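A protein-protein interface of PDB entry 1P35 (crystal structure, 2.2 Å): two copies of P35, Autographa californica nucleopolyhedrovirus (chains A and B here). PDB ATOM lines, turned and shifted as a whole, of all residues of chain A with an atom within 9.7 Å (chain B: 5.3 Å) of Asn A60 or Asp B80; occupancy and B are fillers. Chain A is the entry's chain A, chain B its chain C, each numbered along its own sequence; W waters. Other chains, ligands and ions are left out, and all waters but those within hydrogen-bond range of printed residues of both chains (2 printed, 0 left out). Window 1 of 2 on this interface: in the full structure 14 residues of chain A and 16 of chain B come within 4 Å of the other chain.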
ATOM      1  N   ILE A  30     -18.625   1.183 -12.612  1.00  0.00           N
ATOM      2  CA  ILE A  30     -18.253   1.954 -13.795  1.00  0.00           C
ATOM      3  C   ILE A  30     -19.520   2.380 -14.543  1.00  0.00           C
ATOM      4  O   ILE A  30     -20.491   1.573 -14.715  1.00  0.00           O
ATOM      5  CB  ILE A  30     -17.447   1.056 -14.816  1.00  0.00           C
ATOM      6  CG1 ILE A  30     -16.119   0.635 -14.248  1.00  0.00           C
ATOM      7  CG2 ILE A  30     -17.181   1.779 -16.131  1.00  0.00           C
ATOM      8  CD1 ILE A  30     -15.929  -0.916 -14.434  1.00  0.00           C
ATOM      9  N   ARG A  57      -7.360   0.439  -7.047  1.00  0.00           N
ATOM     10  CA  ARG A  57      -7.061   0.811  -8.435  1.00  0.00           C
ATOM     11  C   ARG A  57      -7.071  -0.505  -9.191  1.00  0.00           C
ATOM     12  O   ARG A  57      -6.429  -1.479  -8.780  1.00  0.00           O
ATOM     13  CB  ARG A  57      -5.677   1.486  -8.546  1.00  0.00           C
ATOM     14  CG  ARG A  57      -5.220   1.963  -9.979  1.00  0.00           C
ATOM     15  CD  ARG A  57      -6.184   2.961 -10.613  1.00  0.00           C
ATOM     16  NE  ARG A  57      -5.654   3.690 -11.779  1.00  0.00           N
ATOM     17  CZ  ARG A  57      -5.300   3.169 -12.957  1.00  0.00           C
ATOM     18  NH1 ARG A  57      -5.385   1.865 -13.199  1.00  0.00           N
ATOM     19  NH2 ARG A  57      -4.879   3.977 -13.925  1.00  0.00           N
ATOM     20  N   LYS A  58      -7.848  -0.556 -10.269  1.00  0.00           N
ATOM     21  CA  LYS A  58      -7.926  -1.766 -11.072  1.00  0.00           C
ATOM     22  C   LYS A  58      -7.198  -1.512 -12.364  1.00  0.00           C
ATOM     23  O   LYS A  58      -6.953  -0.354 -12.727  1.00  0.00           O
ATOM     24  CB  LYS A  58      -9.393  -2.143 -11.356  1.00  0.00           C
ATOM     25  CG  LYS A  58     -10.274  -2.080 -10.135  1.00  0.00           C
ATOM     26  CD  LYS A  58      -9.751  -2.895  -8.935  1.00  0.00           C
ATOM     27  CE  LYS A  58      -9.604  -4.362  -9.240  1.00  0.00           C
ATOM     28  NZ  LYS A  58      -9.117  -5.065  -8.021  1.00  0.00           N
ATOM     29  N   ASN A  59      -6.886  -2.595 -13.072  1.00  0.00           N
ATOM     30  CA  ASN A  59      -6.166  -2.498 -14.345  1.00  0.00           C
ATOM     31  C   ASN A  59      -7.104  -1.898 -15.387  1.00  0.00           C
ATOM     32  O   ASN A  59      -8.324  -1.975 -15.232  1.00  0.00           O
ATOM     33  CB  ASN A  59      -5.639  -3.893 -14.745  1.00  0.00           C
ATOM     34  CG  ASN A  59      -6.725  -4.828 -15.290  1.00  0.00           C
ATOM     35  OD1 ASN A  59      -7.198  -4.647 -16.406  1.00  0.00           O
ATOM     36  ND2 ASN A  59      -7.082  -5.840 -14.522  1.00  0.00           N
ATOM     37  N   ASN A  60      -6.539  -1.300 -16.437  1.00  0.00           N
ATOM     38  CA  ASN A  60      -7.341  -0.600 -17.429  1.00  0.00           C
ATOM     39  C   ASN A  60      -8.311  -1.472 -18.231  1.00  0.00           C
ATOM     40  O   ASN A  60      -9.138  -0.974 -18.941  1.00  0.00           O
ATOM     41  CB  ASN A  60      -6.427   0.211 -18.410  1.00  0.00           C
ATOM     42  CG  ASN A  60      -5.521   1.228 -17.692  1.00  0.00           C
ATOM     43  OD1 ASN A  60      -5.942   1.901 -16.754  1.00  0.00           O
ATOM     44  ND2 ASN A  60      -4.280   1.351 -18.150  1.00  0.00           N
ATOM     45  N   ASN A  61      -8.195  -2.778 -18.119  1.00  0.00           N
ATOM     46  CA  ASN A  61      -9.072  -3.615 -18.889  1.00  0.00           C
ATOM     47  C   ASN A  61     -10.177  -4.283 -18.178  1.00  0.00           C
ATOM     48  O   ASN A  61     -10.988  -4.954 -18.841  1.00  0.00           O
ATOM     49  CB  ASN A  61      -8.301  -4.687 -19.618  1.00  0.00           C
ATOM     50  CG  ASN A  61      -7.871  -4.214 -20.915  1.00  0.00           C
ATOM     51  OD1 ASN A  61      -8.364  -3.174 -21.360  1.00  0.00           O
ATOM     52  ND2 ASN A  61      -6.972  -4.955 -21.574  1.00  0.00           N
ATOM     53  N   LEU A  62     -10.220  -4.110 -16.855  1.00  0.00           N
ATOM     54  CA  LEU A  62     -11.260  -4.763 -16.062  1.00  0.00           C
ATOM     55  C   LEU A  62     -12.696  -4.551 -16.565  1.00  0.00           C
ATOM     56  O   LEU A  62     -13.523  -5.484 -16.584  1.00  0.00           O
ATOM     57  CB  LEU A  62     -11.184  -4.316 -14.622  1.00  0.00           C
ATOM     58  CG  LEU A  62     -12.105  -5.174 -13.741  1.00  0.00           C
ATOM     59  CD1 LEU A  62     -11.765  -6.645 -13.992  1.00  0.00           C
ATOM     60  CD2 LEU A  62     -11.895  -4.846 -12.252  1.00  0.00           C
ATOM     61  N   ARG A  63     -12.964  -3.313 -16.957  1.00  0.00           N
ATOM     62  CA  ARG A  63     -14.242  -2.897 -17.431  1.00  0.00           C
ATOM     63  C   ARG A  63     -14.781  -3.837 -18.514  1.00  0.00           C
ATOM     64  O   ARG A  63     -15.891  -4.346 -18.413  1.00  0.00           O
ATOM     65  CB  ARG A  63     -14.140  -1.481 -18.015  1.00  0.00           C
ATOM     66  CG  ARG A  63     -15.427  -1.140 -18.809  1.00  0.00           C
ATOM     67  CD  ARG A  63     -15.384   0.162 -19.608  1.00  0.00           C
ATOM     68  NE  ARG A  63     -16.686   0.543 -20.193  1.00  0.00           N
ATOM     69  CZ  ARG A  63     -17.326  -0.101 -21.174  1.00  0.00           C
ATOM     70  NH1 ARG A  63     -16.803  -1.189 -21.723  1.00  0.00           N
ATOM     71  NH2 ARG A  63     -18.513   0.338 -21.602  1.00  0.00           N
ATOM     72  N   ASP A  64     -13.983  -4.044 -19.559  1.00  0.00           N
ATOM     73  CA  ASP A  64     -14.380  -4.882 -20.674  1.00  0.00           C
ATOM     74  C   ASP A  64     -14.374  -6.364 -20.313  1.00  0.00           C
ATOM     75  O   ASP A  64     -15.089  -7.149 -20.925  1.00  0.00           O
ATOM     76  CB  ASP A  64     -13.480  -4.639 -21.910  1.00  0.00           C
ATOM     77  CG  ASP A  64     -13.772  -3.307 -22.615  1.00  0.00           C
ATOM     78  OD1 ASP A  64     -14.902  -2.794 -22.492  1.00  0.00           O
ATOM     79  OD2 ASP A  64     -12.890  -2.794 -23.324  1.00  0.00           O
ATOM     80  N   ARG A  65     -13.570  -6.758 -19.332  1.00  0.00           N
ATOM     81  CA  ARG A  65     -13.556  -8.162 -18.957  1.00  0.00           C
ATOM     82  C   ARG A  65     -14.830  -8.478 -18.167  1.00  0.00           C
ATOM     83  O   ARG A  65     -15.355  -9.571 -18.283  1.00  0.00           O
ATOM     84  CB  ARG A  65     -12.316  -8.564 -18.116  1.00  0.00           C
ATOM     85  CG  ARG A  65     -10.995  -8.574 -18.867  1.00  0.00           C
ATOM     86  CD  ARG A  65      -9.965  -9.522 -18.192  1.00  0.00           C
ATOM     87  NE  ARG A  65      -9.635  -9.133 -16.831  1.00  0.00           N
ATOM     88  CZ  ARG A  65      -9.003  -8.006 -16.512  1.00  0.00           C
ATOM     89  NH1 ARG A  65      -8.638  -7.169 -17.462  1.00  0.00           N
ATOM     90  NH2 ARG A  65      -8.742  -7.716 -15.252  1.00  0.00           N
ATOM     91  N   ILE A  66     -15.315  -7.534 -17.358  1.00  0.00           N
ATOM     92  CA  ILE A  66     -16.544  -7.777 -16.599  1.00  0.00           C
ATOM     93  C   ILE A  66     -17.663  -7.957 -17.650  1.00  0.00           C
ATOM     94  O   ILE A  66     -18.326  -8.966 -17.721  1.00  0.00           O
ATOM     95  CB  ILE A  66     -16.885  -6.570 -15.701  1.00  0.00           C
ATOM     96  CG1 ILE A  66     -15.808  -6.425 -14.604  1.00  0.00           C
ATOM     97  CG2 ILE A  66     -18.274  -6.773 -15.049  1.00  0.00           C
ATOM     98  CD1 ILE A  66     -15.912  -5.133 -13.879  1.00  0.00           C
ATOM     99  N   LYS A  93      -9.866   3.370 -28.579  1.00  0.00           N
ATOM    100  CA  LYS A  93      -9.815   3.794 -27.181  1.00  0.00           C
ATOM    101  C   LYS A  93      -8.994   5.081 -27.156  1.00  0.00           C
ATOM    102  O   LYS A  93      -7.870   5.136 -27.653  1.00  0.00           O
ATOM    103  CB  LYS A  93      -9.184   2.715 -26.274  1.00  0.00           C
ATOM    104  CG  LYS A  93     -10.193   1.682 -25.688  1.00  0.00           C
ATOM    105  CD  LYS A  93      -9.493   0.630 -24.823  1.00  0.00           C
ATOM    106  CE  LYS A  93     -10.457  -0.263 -24.040  1.00  0.00           C
ATOM    107  NZ  LYS A  93     -11.384  -1.073 -24.855  1.00  0.00           N
ATOM    108  N   PHE A  95     -10.368   8.145 -24.789  1.00  0.00           N
ATOM    109  CA  PHE A  95     -10.650   8.933 -23.607  1.00  0.00           C
ATOM    110  C   PHE A  95     -10.190   8.192 -22.350  1.00  0.00           C
ATOM    111  O   PHE A  95     -10.543   7.024 -22.150  1.00  0.00           O
ATOM    112  CB  PHE A  95     -12.147   9.240 -23.513  1.00  0.00           C
ATOM    113  CG  PHE A  95     -12.725   9.950 -24.715  1.00  0.00           C
ATOM    114  CD1 PHE A  95     -12.664  11.341 -24.816  1.00  0.00           C
ATOM    115  CD2 PHE A  95     -13.468   9.241 -25.672  1.00  0.00           C
ATOM    116  CE1 PHE A  95     -13.346  12.033 -25.831  1.00  0.00           C
ATOM    117  CE2 PHE A  95     -14.164   9.914 -26.701  1.00  0.00           C
ATOM    118  CZ  PHE A  95     -14.102  11.320 -26.772  1.00  0.00           C
ATOM    119  N   LYS A  96      -9.401   8.855 -21.505  1.00  0.00           N
ATOM    120  CA  LYS A  96      -8.948   8.180 -20.294  1.00  0.00           C
ATOM    121  C   LYS A  96     -10.073   8.092 -19.263  1.00  0.00           C
ATOM    122  O   LYS A  96     -10.937   8.958 -19.202  1.00  0.00           O
ATOM    123  CB  LYS A  96      -7.763   8.906 -19.640  1.00  0.00           C
ATOM    124  CG  LYS A  96      -8.088  10.291 -19.063  1.00  0.00           C
ATOM    125  CD  LYS A  96      -6.897  10.852 -18.256  1.00  0.00           C
ATOM    126  CE  LYS A  96      -6.939  12.388 -18.169  1.00  0.00           C
ATOM    127  NZ  LYS A  96      -8.212  12.935 -17.621  1.00  0.00           N
ATOM    128  N   ASP A  97     -10.059   7.033 -18.468  1.00  0.00           N
ATOM    129  CA  ASP A  97     -11.050   6.891 -17.409  1.00  0.00           C
ATOM    130  C   ASP A  97     -11.010   8.035 -16.391  1.00  0.00           C
ATOM    131  O   ASP A  97      -9.925   8.501 -16.008  1.00  0.00           O
ATOM    132  CB  ASP A  97     -10.816   5.593 -16.620  1.00  0.00           C
ATOM    133  CG  ASP A  97     -10.901   4.352 -17.482  1.00  0.00           C
ATOM    134  OD1 ASP A  97     -11.697   4.338 -18.452  1.00  0.00           O
ATOM    135  OD2 ASP A  97     -10.183   3.375 -17.168  1.00  0.00           O
ATOM    136  N   GLU A  98     -12.189   8.492 -15.950  1.00  0.00           N
ATOM    137  CA  GLU A  98     -12.256   9.526 -14.914  1.00  0.00           C
ATOM    138  C   GLU A  98     -12.582   8.771 -13.610  1.00  0.00           C
ATOM    139  O   GLU A  98     -13.199   7.713 -13.649  1.00  0.00           O
ATOM    140  CB  GLU A  98     -13.345  10.553 -15.201  1.00  0.00           C
ATOM    141  CG  GLU A  98     -13.115  11.477 -16.369  1.00  0.00           C
ATOM    142  CD  GLU A  98     -12.087  12.528 -16.076  1.00  0.00           C
ATOM    143  OE1 GLU A  98     -10.910  12.169 -15.866  1.00  0.00           O
ATOM    144  OE2 GLU A  98     -12.457  13.718 -16.045  1.00  0.00           O
ATOM    145  N   HIS A  99     -12.162   9.302 -12.464  1.00  0.00           N
ATOM    146  CA  HIS A  99     -12.438   8.639 -11.209  1.00  0.00           C
ATOM    147  C   HIS A  99     -13.315   9.436 -10.271  1.00  0.00           C
ATOM    148  O   HIS A  99     -13.086  10.629 -10.047  1.00  0.00           O
ATOM    149  CB  HIS A  99     -11.132   8.285 -10.507  1.00  0.00           C
ATOM    150  CG  HIS A  99     -10.271   7.356 -11.302  1.00  0.00           C
ATOM    151  ND1 HIS A  99      -9.571   7.761 -12.421  1.00  0.00           N
ATOM    152  CD2 HIS A  99     -10.026   6.033 -11.165  1.00  0.00           C
ATOM    153  CE1 HIS A  99      -8.928   6.728 -12.933  1.00  0.00           C
ATOM    154  NE2 HIS A  99      -9.187   5.667 -12.189  1.00  0.00           N
ATOM    155  N   ASN A 163     -15.323   6.861 -19.526  1.00  0.00           N
ATOM    156  CA  ASN A 163     -15.983   5.986 -18.563  1.00  0.00           C
ATOM    157  C   ASN A 163     -15.632   6.663 -17.233  1.00  0.00           C
ATOM    158  O   ASN A 163     -14.478   7.167 -17.075  1.00  0.00           O
ATOM    159  CB  ASN A 163     -15.380   4.581 -18.523  1.00  0.00           C
ATOM    160  CG  ASN A 163     -15.843   3.705 -19.687  1.00  0.00           C
ATOM    161  OD1 ASN A 163     -17.032   3.523 -19.912  1.00  0.00           O
ATOM    162  ND2 ASN A 163     -14.894   3.158 -20.410  1.00  0.00           N
ATOM    163  N   VAL A 165     -15.169   5.924 -13.362  1.00  0.00           N
ATOM    164  CA  VAL A 165     -14.955   4.691 -12.624  1.00  0.00           C
ATOM    165  C   VAL A 165     -14.631   4.862 -11.138  1.00  0.00           C
ATOM    166  O   VAL A 165     -14.300   5.963 -10.670  1.00  0.00           O
ATOM    167  CB  VAL A 165     -13.835   3.872 -13.336  1.00  0.00           C
ATOM    168  CG1 VAL A 165     -14.061   3.889 -14.869  1.00  0.00           C
ATOM    169  CG2 VAL A 165     -12.441   4.525 -13.084  1.00  0.00           C
ATOM    170  N   GLU B  78      -3.871  -7.983 -21.890  1.00  0.00           N
ATOM    171  CA  GLU B  78      -3.113  -7.303 -20.864  1.00  0.00           C
ATOM    172  C   GLU B  78      -3.816  -6.790 -19.610  1.00  0.00           C
ATOM    173  O   GLU B  78      -5.020  -6.612 -19.574  1.00  0.00           O
ATOM    174  CB  GLU B  78      -2.342  -6.149 -21.549  1.00  0.00           C
ATOM    175  CG  GLU B  78      -1.637  -6.624 -22.844  1.00  0.00           C
ATOM    176  CD  GLU B  78      -0.506  -5.716 -23.353  1.00  0.00           C
ATOM    177  OE1 GLU B  78      -0.571  -4.476 -23.148  1.00  0.00           O
ATOM    178  OE2 GLU B  78       0.434  -6.267 -24.002  1.00  0.00           O
ATOM    179  N   ARG B  79      -3.023  -6.587 -18.573  1.00  0.00           N
ATOM    180  CA  ARG B  79      -3.485  -6.019 -17.311  1.00  0.00           C
ATOM    181  C   ARG B  79      -2.464  -4.887 -17.091  1.00  0.00           C
ATOM    182  O   ARG B  79      -1.353  -5.087 -16.593  1.00  0.00           O
ATOM    183  CB  ARG B  79      -3.425  -7.065 -16.178  1.00  0.00           C
ATOM    184  CG  ARG B  79      -4.561  -8.127 -16.217  1.00  0.00           C
ATOM    185  CD  ARG B  79      -4.216  -9.246 -15.238  1.00  0.00           C
ATOM    186  NE  ARG B  79      -4.186  -8.781 -13.858  1.00  0.00           N
ATOM    187  CZ  ARG B  79      -5.221  -8.793 -13.024  1.00  0.00           C
ATOM    188  NH1 ARG B  79      -6.405  -9.254 -13.419  1.00  0.00           N
ATOM    189  NH2 ARG B  79      -5.070  -8.342 -11.788  1.00  0.00           N
ATOM    190  N   ASP B  80      -2.830  -3.700 -17.522  1.00  0.00           N
ATOM    191  CA  ASP B  80      -1.930  -2.554 -17.411  1.00  0.00           C
ATOM    192  C   ASP B  80      -2.452  -1.603 -16.354  1.00  0.00           C
ATOM    193  O   ASP B  80      -3.620  -1.290 -16.334  1.00  0.00           O
ATOM    194  CB  ASP B  80      -1.890  -1.849 -18.756  1.00  0.00           C
ATOM    195  CG  ASP B  80      -0.854  -0.757 -18.813  1.00  0.00           C
ATOM    196  OD1 ASP B  80      -0.750   0.003 -17.852  1.00  0.00           O
ATOM    197  OD2 ASP B  80      -0.183  -0.648 -19.856  1.00  0.00           O
ATOM    198  N   TYR B  81      -1.605  -1.150 -15.439  1.00  0.00           N
ATOM    199  CA  TYR B  81      -2.105  -0.221 -14.456  1.00  0.00           C
ATOM    200  C   TYR B  81      -1.600   1.197 -14.661  1.00  0.00           C
ATOM    201  O   TYR B  81      -1.707   2.008 -13.752  1.00  0.00           O
ATOM    202  CB  TYR B  81      -1.760  -0.665 -13.036  1.00  0.00           C
ATOM    203  CG  TYR B  81      -2.455  -1.941 -12.597  1.00  0.00           C
ATOM    204  CD1 TYR B  81      -1.979  -3.178 -13.007  1.00  0.00           C
ATOM    205  CD2 TYR B  81      -3.537  -1.913 -11.710  1.00  0.00           C
ATOM    206  CE1 TYR B  81      -2.537  -4.351 -12.543  1.00  0.00           C
ATOM    207  CE2 TYR B  81      -4.104  -3.098 -11.237  1.00  0.00           C
ATOM    208  CZ  TYR B  81      -3.582  -4.312 -11.664  1.00  0.00           C
ATOM    209  OH  TYR B  81      -4.040  -5.522 -11.197  1.00  0.00           O
ATOM    210  N   SER B  82      -1.079   1.495 -15.850  1.00  0.00           N
ATOM    211  CA  SER B  82      -0.520   2.822 -16.173  1.00  0.00           C
ATOM    212  C   SER B  82      -1.545   3.958 -16.204  1.00  0.00           C
ATOM    213  O   SER B  82      -2.742   3.720 -16.311  1.00  0.00           O
ATOM    214  CB  SER B  82       0.159   2.790 -17.545  1.00  0.00           C
ATOM    215  OG  SER B  82       1.053   1.685 -17.675  1.00  0.00           O
ATOM    216  N   GLN B  84      -2.221   6.667 -18.571  1.00  0.00           N
ATOM    217  CA  GLN B  84      -1.920   7.244 -19.874  1.00  0.00           C
ATOM    218  C   GLN B  84      -2.995   8.274 -20.210  1.00  0.00           C
ATOM    219  O   GLN B  84      -4.196   7.959 -20.214  1.00  0.00           O
ATOM    220  CB  GLN B  84      -1.830   6.112 -20.902  1.00  0.00           C
ATOM    221  CG  GLN B  84      -0.785   5.065 -20.463  1.00  0.00           C
ATOM    222  CD  GLN B  84      -0.969   3.711 -21.136  1.00  0.00           C
ATOM    223  OE1 GLN B  84      -2.090   3.371 -21.551  1.00  0.00           O
ATOM    224  NE2 GLN B  84       0.114   2.908 -21.205  1.00  0.00           N
ATOM    225  N   TRP B 261       0.485  -7.201 -12.977  1.00  0.00           N
ATOM    226  CA  TRP B 261       0.662  -6.678 -14.320  1.00  0.00           C
ATOM    227  C   TRP B 261       0.895  -7.823 -15.289  1.00  0.00           C
ATOM    228  O   TRP B 261       1.445  -8.858 -14.932  1.00  0.00           O
ATOM    229  CB  TRP B 261       1.891  -5.704 -14.415  1.00  0.00           C
ATOM    230  CG  TRP B 261       1.851  -4.486 -13.500  1.00  0.00           C
ATOM    231  CD1 TRP B 261       1.817  -4.485 -12.097  1.00  0.00           C
ATOM    232  CD2 TRP B 261       1.806  -3.102 -13.900  1.00  0.00           C
ATOM    233  NE1 TRP B 261       1.751  -3.184 -11.637  1.00  0.00           N
ATOM    234  CE2 TRP B 261       1.741  -2.320 -12.710  1.00  0.00           C
ATOM    235  CE3 TRP B 261       1.809  -2.453 -15.139  1.00  0.00           C
ATOM    236  CZ2 TRP B 261       1.682  -0.915 -12.727  1.00  0.00           C
ATOM    237  CZ3 TRP B 261       1.747  -1.009 -15.167  1.00  0.00           C
ATOM    238  CH2 TRP B 261       1.686  -0.275 -13.961  1.00  0.00           C
ATOM    239  N   LYS B 262       0.448  -7.630 -16.520  1.00  0.00           N
ATOM    240  CA  LYS B 262       0.636  -8.608 -17.584  1.00  0.00           C
ATOM    241  C   LYS B 262       0.686  -7.689 -18.805  1.00  0.00           C
ATOM    242  O   LYS B 262      -0.340  -7.143 -19.234  1.00  0.00           O
ATOM    243  CB  LYS B 262      -0.552  -9.584 -17.639  1.00  0.00           C
ATOM    244  CG  LYS B 262      -0.406 -10.707 -18.739  1.00  0.00           C
ATOM    245  CD  LYS B 262      -1.617 -11.651 -18.813  1.00  0.00           C
ATOM    246  CE  LYS B 262      -1.424 -12.619 -20.002  1.00  0.00           C
ATOM    247  NZ  LYS B 262      -2.424 -13.645 -19.933  1.00  0.00           N
ATOM    248  N   ILE B 263       1.899  -7.452 -19.302  1.00  0.00           N
ATOM    249  CA  ILE B 263       2.097  -6.517 -20.428  1.00  0.00           C
ATOM    250  C   ILE B 263       3.041  -7.096 -21.471  1.00  0.00           C
ATOM    251  O   ILE B 263       3.507  -8.235 -21.339  1.00  0.00           O
ATOM    252  CB  ILE B 263       2.680  -5.131 -19.928  1.00  0.00           C
ATOM    253  CG1 ILE B 263       4.101  -5.324 -19.382  1.00  0.00           C
ATOM    254  CG2 ILE B 263       1.789  -4.552 -18.787  1.00  0.00           C
ATOM    255  CD1 ILE B 263       4.758  -4.027 -18.945  1.00  0.00           C
HETATM  256  O   HOH W   1      -5.003  -3.663 -18.974  1.00  0.00           O
HETATM  257  O   HOH W   2      -7.230  -7.758 -20.227  1.00  0.00           O
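The backbone carbonyl oxygen (O) of Ser B82 sits at hydrogen-bond distance from the guanidinium group (NH2) of Arg A57 (3.2 Å).
The backbone carbonyl oxygen of Asp B80 lies within hydrogen-bond range of the backbone NH of Asn A60 (2.9 Å).
The backbone carbonyl oxygen (O) of Ser B82 is in hydrogen-bond range of the side-chain amide nitrogen (ND2) of Asn A60 (3.4 Å).
The side-chain amide nitrogen (ND2) of Asn A61 is in hydrogen-bond range of the backbone carbonyl oxygen (O) of Glu B78 (3.2 Å).
The guanidinium group (NH2) of Arg A65 sits close to the guanidinium group (NH1) of Arg B79 (3.3 Å).
OD1 of Asn A59 sits at hydrogen-bond distance from N of Asn A61 (2.7 Å).
The guanidinium group (NH2) of Arg A65 lies close to the side-chain amide nitrogen (ND2) of Asn A59 (2.6 Å).
NZ of Lys A96 lies within salt-bridge range of OE1 of Glu A98 (3.3 Å).
NH2 of Arg B79 lies within hydrogen-bond range of OH of Tyr B81, at 3.1 Å.
The backbone carbonyl oxygen (O) of Lys B262 sits at hydrogen-bond distance from the backbone NH (N) of Arg B79 (2.8 Å).
The side-chain hydroxyl of Ser B82 sits at hydrogen-bond distance from the side-chain carboxylate of Asp B80.
Among the printed residues, pairs that only touch across the chains: Arg A57 with Tyr B81 (3.7 Å), Lys A58 with Tyr B81 (3.7 Å), Asn A59 with Arg B79 (3.7 Å), Asn A59 with Asp B80 (3.4 Å), Asn A59 with Tyr B81 (3.4 Å) and Lys A96 with Gln B84 (3.7 Å).
Asn A60 touches just these residues of chain B: Asp B80 (2.9 Å) and Ser B82 (3.4 Å).
Asp B80 touches two residues of chain A.
Ser B82 touches just these residues of chain A: Arg A57 (3.2 Å) and Asn A60 (3.4 Å).
Of the printed residues of chain A, Arg B79 touches Asn A59 and Arg A65.
Printed residues of chain B within 4 Å of Lys A58: Tyr B81 (3.7 Å).
Printed residues of chain B within 4 Å of Arg A57: Tyr B81 and Ser B82.
Of the printed residues of chain A, Gln B84 touches Lys A96.
Asn A163 touches none of the printed residues of chain B.
Lys A93 touches none of the printed residues of chain B.
Printed residues of chain A that touch a printed residue of chain B: Arg A57, Lys A58, Asn A59, Asn A60, Asn A61, Arg A65 and Lys A96.
Hydrophobic or aromatic side chains of chain B that line the printed part of chain A: Tyr B81.
Among the printed residues, 11 pairs touch across the chains.
No position is printed for both chains.
Water W2 lies within hydrogen-bond range of O of Glu B78, ND2 of Asn A61 and NH1 of Arg A65.
Water W1 lies within hydrogen-bond range of N of Asp B80, O of Glu B78 and N of Asn A61.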
